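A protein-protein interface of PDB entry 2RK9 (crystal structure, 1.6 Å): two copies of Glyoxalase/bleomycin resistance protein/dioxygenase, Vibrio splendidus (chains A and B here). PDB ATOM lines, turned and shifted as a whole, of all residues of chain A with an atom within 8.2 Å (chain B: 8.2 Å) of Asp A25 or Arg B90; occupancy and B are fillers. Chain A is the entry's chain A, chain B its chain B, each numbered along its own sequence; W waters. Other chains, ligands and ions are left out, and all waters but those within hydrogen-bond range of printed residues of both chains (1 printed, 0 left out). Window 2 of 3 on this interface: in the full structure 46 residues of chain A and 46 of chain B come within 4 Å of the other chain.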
ATOM      1  N   ASN A  17       0.304  21.507  10.828  1.00  0.00           N
ATOM      2  CA  ASN A  17       0.753  20.165  10.473  1.00  0.00           C
ATOM      3  C   ASN A  17      -0.262  19.103  10.878  1.00  0.00           C
ATOM      4  O   ASN A  17      -0.431  18.097  10.196  1.00  0.00           O
ATOM      5  CB  ASN A  17       2.122  19.873  11.094  1.00  0.00           C
ATOM      6  CG  ASN A  17       3.240  20.672  10.429  1.00  0.00           C
ATOM      7  OD1 ASN A  17       3.290  20.779   9.206  1.00  0.00           O
ATOM      8  ND2 ASN A  17       4.140  21.228  11.228  1.00  0.00           N
ATOM      9  N   VAL A  18      -0.949  19.330  11.991  1.00  0.00           N
ATOM     10  CA  VAL A  18      -1.959  18.389  12.452  1.00  0.00           C
ATOM     11  C   VAL A  18      -3.139  18.401  11.492  1.00  0.00           C
ATOM     12  O   VAL A  18      -3.679  17.357  11.136  1.00  0.00           O
ATOM     13  CB  VAL A  18      -2.461  18.767  13.861  1.00  0.00           C
ATOM     14  CG1 VAL A  18      -3.743  18.020  14.187  1.00  0.00           C
ATOM     15  CG2 VAL A  18      -1.390  18.447  14.883  1.00  0.00           C
ATOM     16  N   SER A  19      -3.529  19.597  11.074  1.00  0.00           N
ATOM     17  CA  SER A  19      -4.655  19.752  10.161  1.00  0.00           C
ATOM     18  C   SER A  19      -4.310  19.244   8.766  1.00  0.00           C
ATOM     19  O   SER A  19      -5.120  18.579   8.123  1.00  0.00           O
ATOM     20  CB  SER A  19      -5.072  21.222  10.100  1.00  0.00           C
ATOM     21  OG  SER A  19      -5.377  21.709  11.397  1.00  0.00           O
ATOM     22  N   GLN A  20      -3.105  19.550   8.295  1.00  0.00           N
ATOM     23  CA  GLN A  20      -2.704  19.091   6.972  1.00  0.00           C
ATOM     24  C   GLN A  20      -2.661  17.563   6.917  1.00  0.00           C
ATOM     25  O   GLN A  20      -3.125  16.954   5.951  1.00  0.00           O
ATOM     26  CB  GLN A  20      -1.337  19.657   6.596  1.00  0.00           C
ATOM     27  CG  GLN A  20      -0.926  19.320   5.171  1.00  0.00           C
ATOM     28  CD  GLN A  20       0.357  20.010   4.748  1.00  0.00           C
ATOM     29  OE1 GLN A  20       0.566  21.186   5.040  1.00  0.00           O
ATOM     30  NE2 GLN A  20       1.214  19.283   4.035  1.00  0.00           N
ATOM     31  N   SER A  21      -2.112  16.940   7.956  1.00  0.00           N
ATOM     32  CA  SER A  21      -2.029  15.485   8.010  1.00  0.00           C
ATOM     33  C   SER A  21      -3.403  14.832   8.017  1.00  0.00           C
ATOM     34  O   SER A  21      -3.610  13.792   7.388  1.00  0.00           O
ATOM     35  CB  SER A  21      -1.272  15.039   9.262  1.00  0.00           C
ATOM     36  OG  SER A  21       0.047  15.552   9.260  1.00  0.00           O
ATOM     37  N   PHE A  22      -4.342  15.432   8.739  1.00  0.00           N
ATOM     38  CA  PHE A  22      -5.683  14.881   8.811  1.00  0.00           C
ATOM     39  C   PHE A  22      -6.271  14.864   7.409  1.00  0.00           C
ATOM     40  O   PHE A  22      -6.744  13.841   6.942  1.00  0.00           O
ATOM     41  CB  PHE A  22      -6.575  15.732   9.710  1.00  0.00           C
ATOM     42  CG  PHE A  22      -7.899  15.098  10.009  1.00  0.00           C
ATOM     43  CD1 PHE A  22      -8.000  14.106  10.978  1.00  0.00           C
ATOM     44  CD2 PHE A  22      -9.038  15.466   9.302  1.00  0.00           C
ATOM     45  CE1 PHE A  22      -9.219  13.484  11.242  1.00  0.00           C
ATOM     46  CE2 PHE A  22     -10.267  14.850   9.555  1.00  0.00           C
ATOM     47  CZ  PHE A  22     -10.354  13.858  10.526  1.00  0.00           C
ATOM     48  N   PHE A  23      -6.229  16.015   6.748  1.00  0.00           N
ATOM     49  CA  PHE A  23      -6.757  16.150   5.400  1.00  0.00           C
ATOM     50  C   PHE A  23      -6.069  15.245   4.381  1.00  0.00           C
ATOM     51  O   PHE A  23      -6.734  14.642   3.542  1.00  0.00           O
ATOM     52  CB  PHE A  23      -6.661  17.613   4.955  1.00  0.00           C
ATOM     53  CG  PHE A  23      -7.851  18.445   5.343  1.00  0.00           C
ATOM     54  CD1 PHE A  23      -8.930  18.577   4.472  1.00  0.00           C
ATOM     55  CD2 PHE A  23      -7.900  19.098   6.574  1.00  0.00           C
ATOM     56  CE1 PHE A  23     -10.043  19.346   4.823  1.00  0.00           C
ATOM     57  CE2 PHE A  23      -9.008  19.866   6.931  1.00  0.00           C
ATOM     58  CZ  PHE A  23     -10.078  19.991   6.054  1.00  0.00           C
ATOM     59  N   VAL A  24      -4.744  15.152   4.449  1.00  0.00           N
ATOM     60  CA  VAL A  24      -3.999  14.320   3.503  1.00  0.00           C
ATOM     61  C   VAL A  24      -4.024  12.832   3.840  1.00  0.00           C
ATOM     62  O   VAL A  24      -4.439  12.010   3.018  1.00  0.00           O
ATOM     63  CB  VAL A  24      -2.523  14.774   3.397  1.00  0.00           C
ATOM     64  CG1 VAL A  24      -1.747  13.830   2.478  1.00  0.00           C
ATOM     65  CG2 VAL A  24      -2.459  16.198   2.857  1.00  0.00           C
ATOM     66  N   ASP A  25      -3.588  12.490   5.051  1.00  0.00           N
ATOM     67  CA  ASP A  25      -3.536  11.096   5.481  1.00  0.00           C
ATOM     68  C   ASP A  25      -4.888  10.451   5.763  1.00  0.00           C
ATOM     69  O   ASP A  25      -5.152   9.330   5.320  1.00  0.00           O
ATOM     70  CB  ASP A  25      -2.652  10.960   6.727  1.00  0.00           C
ATOM     71  CG  ASP A  25      -1.235  11.456   6.495  1.00  0.00           C
ATOM     72  OD1 ASP A  25      -0.698  11.212   5.392  1.00  0.00           O
ATOM     73  OD2 ASP A  25      -0.655  12.082   7.411  1.00  0.00           O
ATOM     74  N   VAL A  26      -5.744  11.144   6.505  1.00  0.00           N
ATOM     75  CA  VAL A  26      -7.045  10.586   6.841  1.00  0.00           C
ATOM     76  C   VAL A  26      -8.081  10.743   5.727  1.00  0.00           C
ATOM     77  O   VAL A  26      -8.705   9.765   5.310  1.00  0.00           O
ATOM     78  CB  VAL A  26      -7.609  11.221   8.147  1.00  0.00           C
ATOM     79  CG1 VAL A  26      -8.987  10.637   8.463  1.00  0.00           C
ATOM     80  CG2 VAL A  26      -6.653  10.961   9.316  1.00  0.00           C
ATOM     81  N   LEU A  27      -8.263  11.964   5.234  1.00  0.00           N
ATOM     82  CA  LEU A  27      -9.264  12.191   4.197  1.00  0.00           C
ATOM     83  C   LEU A  27      -8.787  11.955   2.772  1.00  0.00           C
ATOM     84  O   LEU A  27      -9.599  11.916   1.842  1.00  0.00           O
ATOM     85  CB  LEU A  27      -9.837  13.602   4.330  1.00  0.00           C
ATOM     86  CG  LEU A  27     -10.452  13.903   5.700  1.00  0.00           C
ATOM     87  CD1 LEU A  27     -10.853  15.374   5.785  1.00  0.00           C
ATOM     88  CD2 LEU A  27     -11.648  13.003   5.932  1.00  0.00           C
ATOM     89  N   GLY A  28      -7.478  11.816   2.588  1.00  0.00           N
ATOM     90  CA  GLY A  28      -6.956  11.564   1.257  1.00  0.00           C
ATOM     91  C   GLY A  28      -6.873  12.746   0.309  1.00  0.00           C
ATOM     92  O   GLY A  28      -6.821  12.554  -0.905  1.00  0.00           O
ATOM     93  N   PHE A  29      -6.868  13.964   0.845  1.00  0.00           N
ATOM     94  CA  PHE A  29      -6.766  15.164   0.015  1.00  0.00           C
ATOM     95  C   PHE A  29      -5.348  15.280  -0.534  1.00  0.00           C
ATOM     96  O   PHE A  29      -4.405  14.728   0.030  1.00  0.00           O
ATOM     97  CB  PHE A  29      -7.052  16.433   0.834  1.00  0.00           C
ATOM     98  CG  PHE A  29      -8.514  16.736   1.035  1.00  0.00           C
ATOM     99  CD1 PHE A  29      -9.022  17.983   0.686  1.00  0.00           C
ATOM    100  CD2 PHE A  29      -9.369  15.803   1.620  1.00  0.00           C
ATOM    101  CE1 PHE A  29     -10.362  18.298   0.919  1.00  0.00           C
ATOM    102  CE2 PHE A  29     -10.706  16.109   1.858  1.00  0.00           C
ATOM    103  CZ  PHE A  29     -11.204  17.358   1.509  1.00  0.00           C
ATOM    104  N   GLU A  30      -5.195  16.007  -1.634  1.00  0.00           N
ATOM    105  CA  GLU A  30      -3.870  16.212  -2.190  1.00  0.00           C
ATOM    106  C   GLU A  30      -3.484  17.683  -2.085  1.00  0.00           C
ATOM    107  O   GLU A  30      -4.309  18.571  -2.296  1.00  0.00           O
ATOM    108  CB  GLU A  30      -3.796  15.774  -3.656  1.00  0.00           C
ATOM    109  CG  GLU A  30      -2.485  16.212  -4.310  1.00  0.00           C
ATOM    110  CD  GLU A  30      -2.183  15.516  -5.623  1.00  0.00           C
ATOM    111  OE1 GLU A  30      -3.095  15.430  -6.485  1.00  0.00           O
ATOM    112  OE2 GLU A  30      -1.023  15.064  -5.800  1.00  0.00           O
ATOM    113  N   LEU A  43      -5.476  22.761  -0.793  1.00  0.00           N
ATOM    114  CA  LEU A  43      -5.768  21.357  -1.035  1.00  0.00           C
ATOM    115  C   LEU A  43      -6.966  21.116  -1.941  1.00  0.00           C
ATOM    116  O   LEU A  43      -7.767  22.019  -2.202  1.00  0.00           O
ATOM    117  CB  LEU A  43      -6.005  20.647   0.294  1.00  0.00           C
ATOM    118  CG  LEU A  43      -4.828  20.733   1.265  1.00  0.00           C
ATOM    119  CD1 LEU A  43      -5.202  21.579   2.469  1.00  0.00           C
ATOM    120  CD2 LEU A  43      -4.431  19.339   1.692  1.00  0.00           C
ATOM    121  N   LEU A  45      -9.732  17.679  -3.346  1.00  0.00           N
ATOM    122  CA  LEU A  45     -10.165  16.298  -3.303  1.00  0.00           C
ATOM    123  C   LEU A  45     -10.972  16.137  -4.578  1.00  0.00           C
ATOM    124  O   LEU A  45     -12.133  16.540  -4.650  1.00  0.00           O
ATOM    125  CB  LEU A  45     -11.039  16.005  -2.081  1.00  0.00           C
ATOM    126  CG  LEU A  45     -11.319  14.501  -1.948  1.00  0.00           C
ATOM    127  CD1 LEU A  45     -10.011  13.767  -1.728  1.00  0.00           C
ATOM    128  CD2 LEU A  45     -12.276  14.231  -0.806  1.00  0.00           C
ATOM    129  N   ASP B  83     -16.245   8.657  -4.664  1.00  0.00           N
ATOM    130  CA  ASP B  83     -16.389   7.298  -4.144  1.00  0.00           C
ATOM    131  C   ASP B  83     -16.352   7.350  -2.617  1.00  0.00           C
ATOM    132  O   ASP B  83     -15.289   7.219  -2.015  1.00  0.00           O
ATOM    133  CB  ASP B  83     -15.228   6.446  -4.652  1.00  0.00           C
ATOM    134  CG  ASP B  83     -15.667   5.098  -5.159  1.00  0.00           C
ATOM    135  OD1 ASP B  83     -16.574   4.487  -4.552  1.00  0.00           O
ATOM    136  OD2 ASP B  83     -15.085   4.643  -6.167  1.00  0.00           O
ATOM    137  N   ILE B  84     -17.520   7.511  -2.000  1.00  0.00           N
ATOM    138  CA  ILE B  84     -17.616   7.635  -0.550  1.00  0.00           C
ATOM    139  C   ILE B  84     -17.255   6.392   0.269  1.00  0.00           C
ATOM    140  O   ILE B  84     -16.753   6.511   1.385  1.00  0.00           O
ATOM    141  CB  ILE B  84     -19.025   8.141  -0.156  1.00  0.00           C
ATOM    142  CG1 ILE B  84     -18.981   8.786   1.230  1.00  0.00           C
ATOM    143  CG2 ILE B  84     -20.020   7.000  -0.172  1.00  0.00           C
ATOM    144  CD1 ILE B  84     -20.268   9.525   1.593  1.00  0.00           C
ATOM    145  N   GLU B  85     -17.488   5.204  -0.278  1.00  0.00           N
ATOM    146  CA  GLU B  85     -17.173   3.974   0.439  1.00  0.00           C
ATOM    147  C   GLU B  85     -15.707   3.862   0.867  1.00  0.00           C
ATOM    148  O   GLU B  85     -15.420   3.662   2.050  1.00  0.00           O
ATOM    149  CB  GLU B  85     -17.562   2.754  -0.402  1.00  0.00           C
ATOM    150  CG  GLU B  85     -19.057   2.483  -0.438  1.00  0.00           C
ATOM    151  CD  GLU B  85     -19.628   2.263   0.943  1.00  0.00           C
ATOM    152  OE1 GLU B  85     -18.902   1.710   1.801  1.00  0.00           O
ATOM    153  OE2 GLU B  85     -20.804   2.624   1.178  1.00  0.00           O
ATOM    154  N   PRO B  86     -14.759   3.981  -0.081  1.00  0.00           N
ATOM    155  CA  PRO B  86     -13.362   3.872   0.355  1.00  0.00           C
ATOM    156  C   PRO B  86     -12.942   5.005   1.293  1.00  0.00           C
ATOM    157  O   PRO B  86     -12.106   4.818   2.170  1.00  0.00           O
ATOM    158  CB  PRO B  86     -12.581   3.860  -0.962  1.00  0.00           C
ATOM    159  CG  PRO B  86     -13.484   4.569  -1.931  1.00  0.00           C
ATOM    160  CD  PRO B  86     -14.853   4.068  -1.549  1.00  0.00           C
ATOM    161  N   LEU B  87     -13.522   6.181   1.102  1.00  0.00           N
ATOM    162  CA  LEU B  87     -13.206   7.307   1.973  1.00  0.00           C
ATOM    163  C   LEU B  87     -13.641   6.977   3.402  1.00  0.00           C
ATOM    164  O   LEU B  87     -12.854   7.089   4.340  1.00  0.00           O
ATOM    165  CB  LEU B  87     -13.928   8.569   1.495  1.00  0.00           C
ATOM    166  CG  LEU B  87     -13.891   9.803   2.404  1.00  0.00           C
ATOM    167  CD1 LEU B  87     -12.459  10.196   2.725  1.00  0.00           C
ATOM    168  CD2 LEU B  87     -14.613  10.950   1.695  1.00  0.00           C
ATOM    169  N   TYR B  88     -14.891   6.556   3.560  1.00  0.00           N
ATOM    170  CA  TYR B  88     -15.412   6.236   4.879  1.00  0.00           C
ATOM    171  C   TYR B  88     -14.639   5.125   5.573  1.00  0.00           C
ATOM    172  O   TYR B  88     -14.396   5.201   6.773  1.00  0.00           O
ATOM    173  CB  TYR B  88     -16.888   5.833   4.804  1.00  0.00           C
ATOM    174  CG  TYR B  88     -17.519   5.605   6.159  1.00  0.00           C
ATOM    175  CD1 TYR B  88     -17.706   6.662   7.046  1.00  0.00           C
ATOM    176  CD2 TYR B  88     -17.941   4.331   6.553  1.00  0.00           C
ATOM    177  CE1 TYR B  88     -18.296   6.462   8.295  1.00  0.00           C
ATOM    178  CE2 TYR B  88     -18.535   4.122   7.804  1.00  0.00           C
ATOM    179  CZ  TYR B  88     -18.708   5.197   8.668  1.00  0.00           C
ATOM    180  OH  TYR B  88     -19.295   5.022   9.905  1.00  0.00           O
ATOM    181  N   GLN B  89     -14.258   4.088   4.835  1.00  0.00           N
ATOM    182  CA  GLN B  89     -13.539   3.001   5.474  1.00  0.00           C
ATOM    183  C   GLN B  89     -12.178   3.454   6.005  1.00  0.00           C
ATOM    184  O   GLN B  89     -11.743   2.991   7.060  1.00  0.00           O
ATOM    185  CB  GLN B  89     -13.416   1.794   4.528  1.00  0.00           C
ATOM    186  CG  GLN B  89     -12.769   2.069   3.209  1.00  0.00           C
ATOM    187  CD  GLN B  89     -12.583   0.795   2.397  1.00  0.00           C
ATOM    188  OE1 GLN B  89     -13.551   0.210   1.893  1.00  0.00           O
ATOM    189  NE2 GLN B  89     -11.332   0.351   2.280  1.00  0.00           N
ATOM    190  N   ARG B  90     -11.527   4.393   5.319  1.00  0.00           N
ATOM    191  CA  ARG B  90     -10.228   4.878   5.787  1.00  0.00           C
ATOM    192  C   ARG B  90     -10.399   5.732   7.038  1.00  0.00           C
ATOM    193  O   ARG B  90      -9.602   5.642   7.972  1.00  0.00           O
ATOM    194  CB  ARG B  90      -9.511   5.685   4.698  1.00  0.00           C
ATOM    195  CG  ARG B  90      -8.085   6.059   5.093  1.00  0.00           C
ATOM    196  CD  ARG B  90      -7.291   6.723   3.968  1.00  0.00           C
ATOM    197  NE  ARG B  90      -7.970   7.898   3.440  1.00  0.00           N
ATOM    198  CZ  ARG B  90      -8.735   7.895   2.353  1.00  0.00           C
ATOM    199  NH1 ARG B  90      -8.918   6.772   1.665  1.00  0.00           N
ATOM    200  NH2 ARG B  90      -9.319   9.017   1.947  1.00  0.00           N
ATOM    201  N   VAL B  91     -11.442   6.559   7.057  1.00  0.00           N
ATOM    202  CA  VAL B  91     -11.709   7.416   8.210  1.00  0.00           C
ATOM    203  C   VAL B  91     -12.040   6.557   9.425  1.00  0.00           C
ATOM    204  O   VAL B  91     -11.564   6.809  10.534  1.00  0.00           O
ATOM    205  CB  VAL B  91     -12.894   8.366   7.931  1.00  0.00           C
ATOM    206  CG1 VAL B  91     -13.248   9.154   9.192  1.00  0.00           C
ATOM    207  CG2 VAL B  91     -12.536   9.313   6.808  1.00  0.00           C
ATOM    208  N   ASN B  92     -12.856   5.535   9.197  1.00  0.00           N
ATOM    209  CA  ASN B  92     -13.282   4.620  10.245  1.00  0.00           C
ATOM    210  C   ASN B  92     -12.087   3.843  10.791  1.00  0.00           C
ATOM    211  O   ASN B  92     -12.061   3.473  11.967  1.00  0.00           O
ATOM    212  CB  ASN B  92     -14.304   3.649   9.665  1.00  0.00           C
ATOM    213  CG  ASN B  92     -15.329   3.188  10.679  1.00  0.00           C
ATOM    214  OD1 ASN B  92     -16.169   2.347  10.359  1.00  0.00           O
ATOM    215  ND2 ASN B  92     -15.279   3.732  11.895  1.00  0.00           N
ATOM    216  N   GLU B  93     -11.101   3.600   9.929  1.00  0.00           N
ATOM    217  CA  GLU B  93      -9.903   2.862  10.315  1.00  0.00           C
ATOM    218  C   GLU B  93      -8.879   3.681  11.083  1.00  0.00           C
ATOM    219  O   GLU B  93      -8.446   3.289  12.165  1.00  0.00           O
ATOM    220  CB  GLU B  93      -9.230   2.256   9.079  1.00  0.00           C
ATOM    221  CG  GLU B  93      -9.794   0.906   8.696  1.00  0.00           C
ATOM    222  CD  GLU B  93      -9.083   0.272   7.520  1.00  0.00           C
ATOM    223  OE1 GLU B  93      -7.832   0.342   7.448  1.00  0.00           O
ATOM    224  OE2 GLU B  93      -9.782  -0.317   6.674  1.00  0.00           O
ATOM    225  N   SER B  94      -8.505   4.831  10.536  1.00  0.00           N
ATOM    226  CA  SER B  94      -7.494   5.666  11.168  1.00  0.00           C
ATOM    227  C   SER B  94      -7.969   6.813  12.052  1.00  0.00           C
ATOM    228  O   SER B  94      -7.149   7.452  12.714  1.00  0.00           O
ATOM    229  CB  SER B  94      -6.554   6.216  10.096  1.00  0.00           C
ATOM    230  OG  SER B  94      -7.298   6.792   9.040  1.00  0.00           O
ATOM    231  N   ALA B  95      -9.272   7.083  12.076  1.00  0.00           N
ATOM    232  CA  ALA B  95      -9.787   8.174  12.902  1.00  0.00           C
ATOM    233  C   ALA B  95     -11.266   8.035  13.236  1.00  0.00           C
ATOM    234  O   ALA B  95     -12.036   8.985  13.092  1.00  0.00           O
ATOM    235  CB  ALA B  95      -9.533   9.512  12.210  1.00  0.00           C
ATOM    236  N   ALA B  96     -11.655   6.854  13.701  1.00  0.00           N
ATOM    237  CA  ALA B  96     -13.045   6.591  14.052  1.00  0.00           C
ATOM    238  C   ALA B  96     -13.618   7.602  15.052  1.00  0.00           C
ATOM    239  O   ALA B  96     -14.793   7.955  14.981  1.00  0.00           O
ATOM    240  CB  ALA B  96     -13.180   5.174  14.601  1.00  0.00           C
ATOM    241  N   ILE B  99     -15.552  10.537  13.567  1.00  0.00           N
ATOM    242  CA  ILE B  99     -16.827  10.364  12.894  1.00  0.00           C
ATOM    243  C   ILE B  99     -17.946  10.968  13.731  1.00  0.00           C
ATOM    244  O   ILE B  99     -18.122  10.621  14.896  1.00  0.00           O
ATOM    245  CB  ILE B  99     -17.099   8.875  12.607  1.00  0.00           C
ATOM    246  CG1 ILE B  99     -16.006   8.338  11.680  1.00  0.00           C
ATOM    247  CG2 ILE B  99     -18.464   8.710  11.952  1.00  0.00           C
ATOM    248  CD1 ILE B  99     -16.103   6.859  11.379  1.00  0.00           C
ATOM    249  N   PHE B 120     -21.804  10.811   5.263  1.00  0.00           N
ATOM    250  CA  PHE B 120     -21.327  10.630   6.619  1.00  0.00           C
ATOM    251  C   PHE B 120     -20.704  11.962   7.002  1.00  0.00           C
ATOM    252  O   PHE B 120     -20.381  12.770   6.135  1.00  0.00           O
ATOM    253  CB  PHE B 120     -20.331   9.461   6.736  1.00  0.00           C
ATOM    254  CG  PHE B 120     -18.936   9.758   6.268  1.00  0.00           C
ATOM    255  CD1 PHE B 120     -17.983  10.252   7.155  1.00  0.00           C
ATOM    256  CD2 PHE B 120     -18.550   9.467   4.965  1.00  0.00           C
ATOM    257  CE1 PHE B 120     -16.660  10.447   6.750  1.00  0.00           C
ATOM    258  CE2 PHE B 120     -17.235   9.658   4.549  1.00  0.00           C
ATOM    259  CZ  PHE B 120     -16.288  10.147   5.444  1.00  0.00           C
HETATM  260  O   HOH W   1     -10.549  10.437  -0.218  1.00  0.00           O
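Hydrophobic or aromatic side chains of chain B within 4 Å of the printed part of chain A: Leu B87, Val B91 and Ala B95. Printed residues of chain A that touch a printed residue of chain B: Asp A25, Val A26, Leu A27 and Gly A28. Hydrophobic or aromatic side chains of chain A within 4 Å of the printed part of chain B: Val A26 and Leu A27. Among the printed residues, 7 pairs touch across the chains. Among the printed residues, no Asp or Glu carboxylate lies within 4 Å of a Lys or Arg side-chain nitrogen of the other chain.
No position is printed for both chains. Of the 7 pairs that touch across the chains among the printed residues, none has its exchanged pair printed and touching as well.
The backbone carbonyl oxygen (O) of Arg B90 is in hydrogen-bond range of the side-chain hydroxyl (OG) of Ser B94 (2.8 Å). The backbone carbonyl oxygen (O) of Phe A23 is in hydrogen-bond range of the backbone NH (N) of Gly A28, at 3.1 Å. The backbone NH (N) of Ala B96 is in hydrogen-bond range of the backbone carbonyl oxygen (O) of Val B91 (3.2 Å). The backbone carbonyl oxygen (O) of Phe A22 is in hydrogen-bond range of the backbone NH (N) of Leu A27, at 3.0 Å.
Among the printed residues, pairs that only touch across the chains: Leu A27 with Leu B87 (3.5 Å), Asp A25 with Arg B90 (3.6 Å), Leu A27 with Val B91 (3.9 Å) and Val A26 with Ala B95 (3.95 Å).
Water W1 bridges the backbone carbonyl oxygen (O) of Leu A27 and the guanidinium group (NH2) of Arg B90.
The backbone NH (N) of Gly A28 sits close to the guanidinium group (NH2) of Arg B90 (3.4 Å). NH2 of Arg B90 is in hydrogen-bond range of O of Leu A27, 2.9 Å away. The guanidinium group of Arg B90 lies within hydrogen-bond range of the backbone carbonyl oxygen of Val A26 (2.7 Å).
Asp A25 touches one residue of chain B. Of chain A, only Asp A25, Val A26, Leu A27 and Gly A28 come within 4 Å of Arg B90. Printed residues of chain A within 4 Å of Leu B87: Leu A27 (3.5 Å). Of the printed residues of chain B, Leu A27 touches Leu B87, Arg B90 and Val B91. Printed residues of chain B within 4 Å of Val A26: Arg B90 and Ala B95. Printed residues of chain B within 4 Å of Gly A28: Arg B90 (3.4 Å). Of the printed residues of chain A, Val B91 touches Leu A27 (3.9 Å). The nearest residue of chain A that does not touch Arg B90 is Val A24 (5.4 Å). The nearest printed residue of chain A that does not touch Val B91 is Val A26 (4.1 Å).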
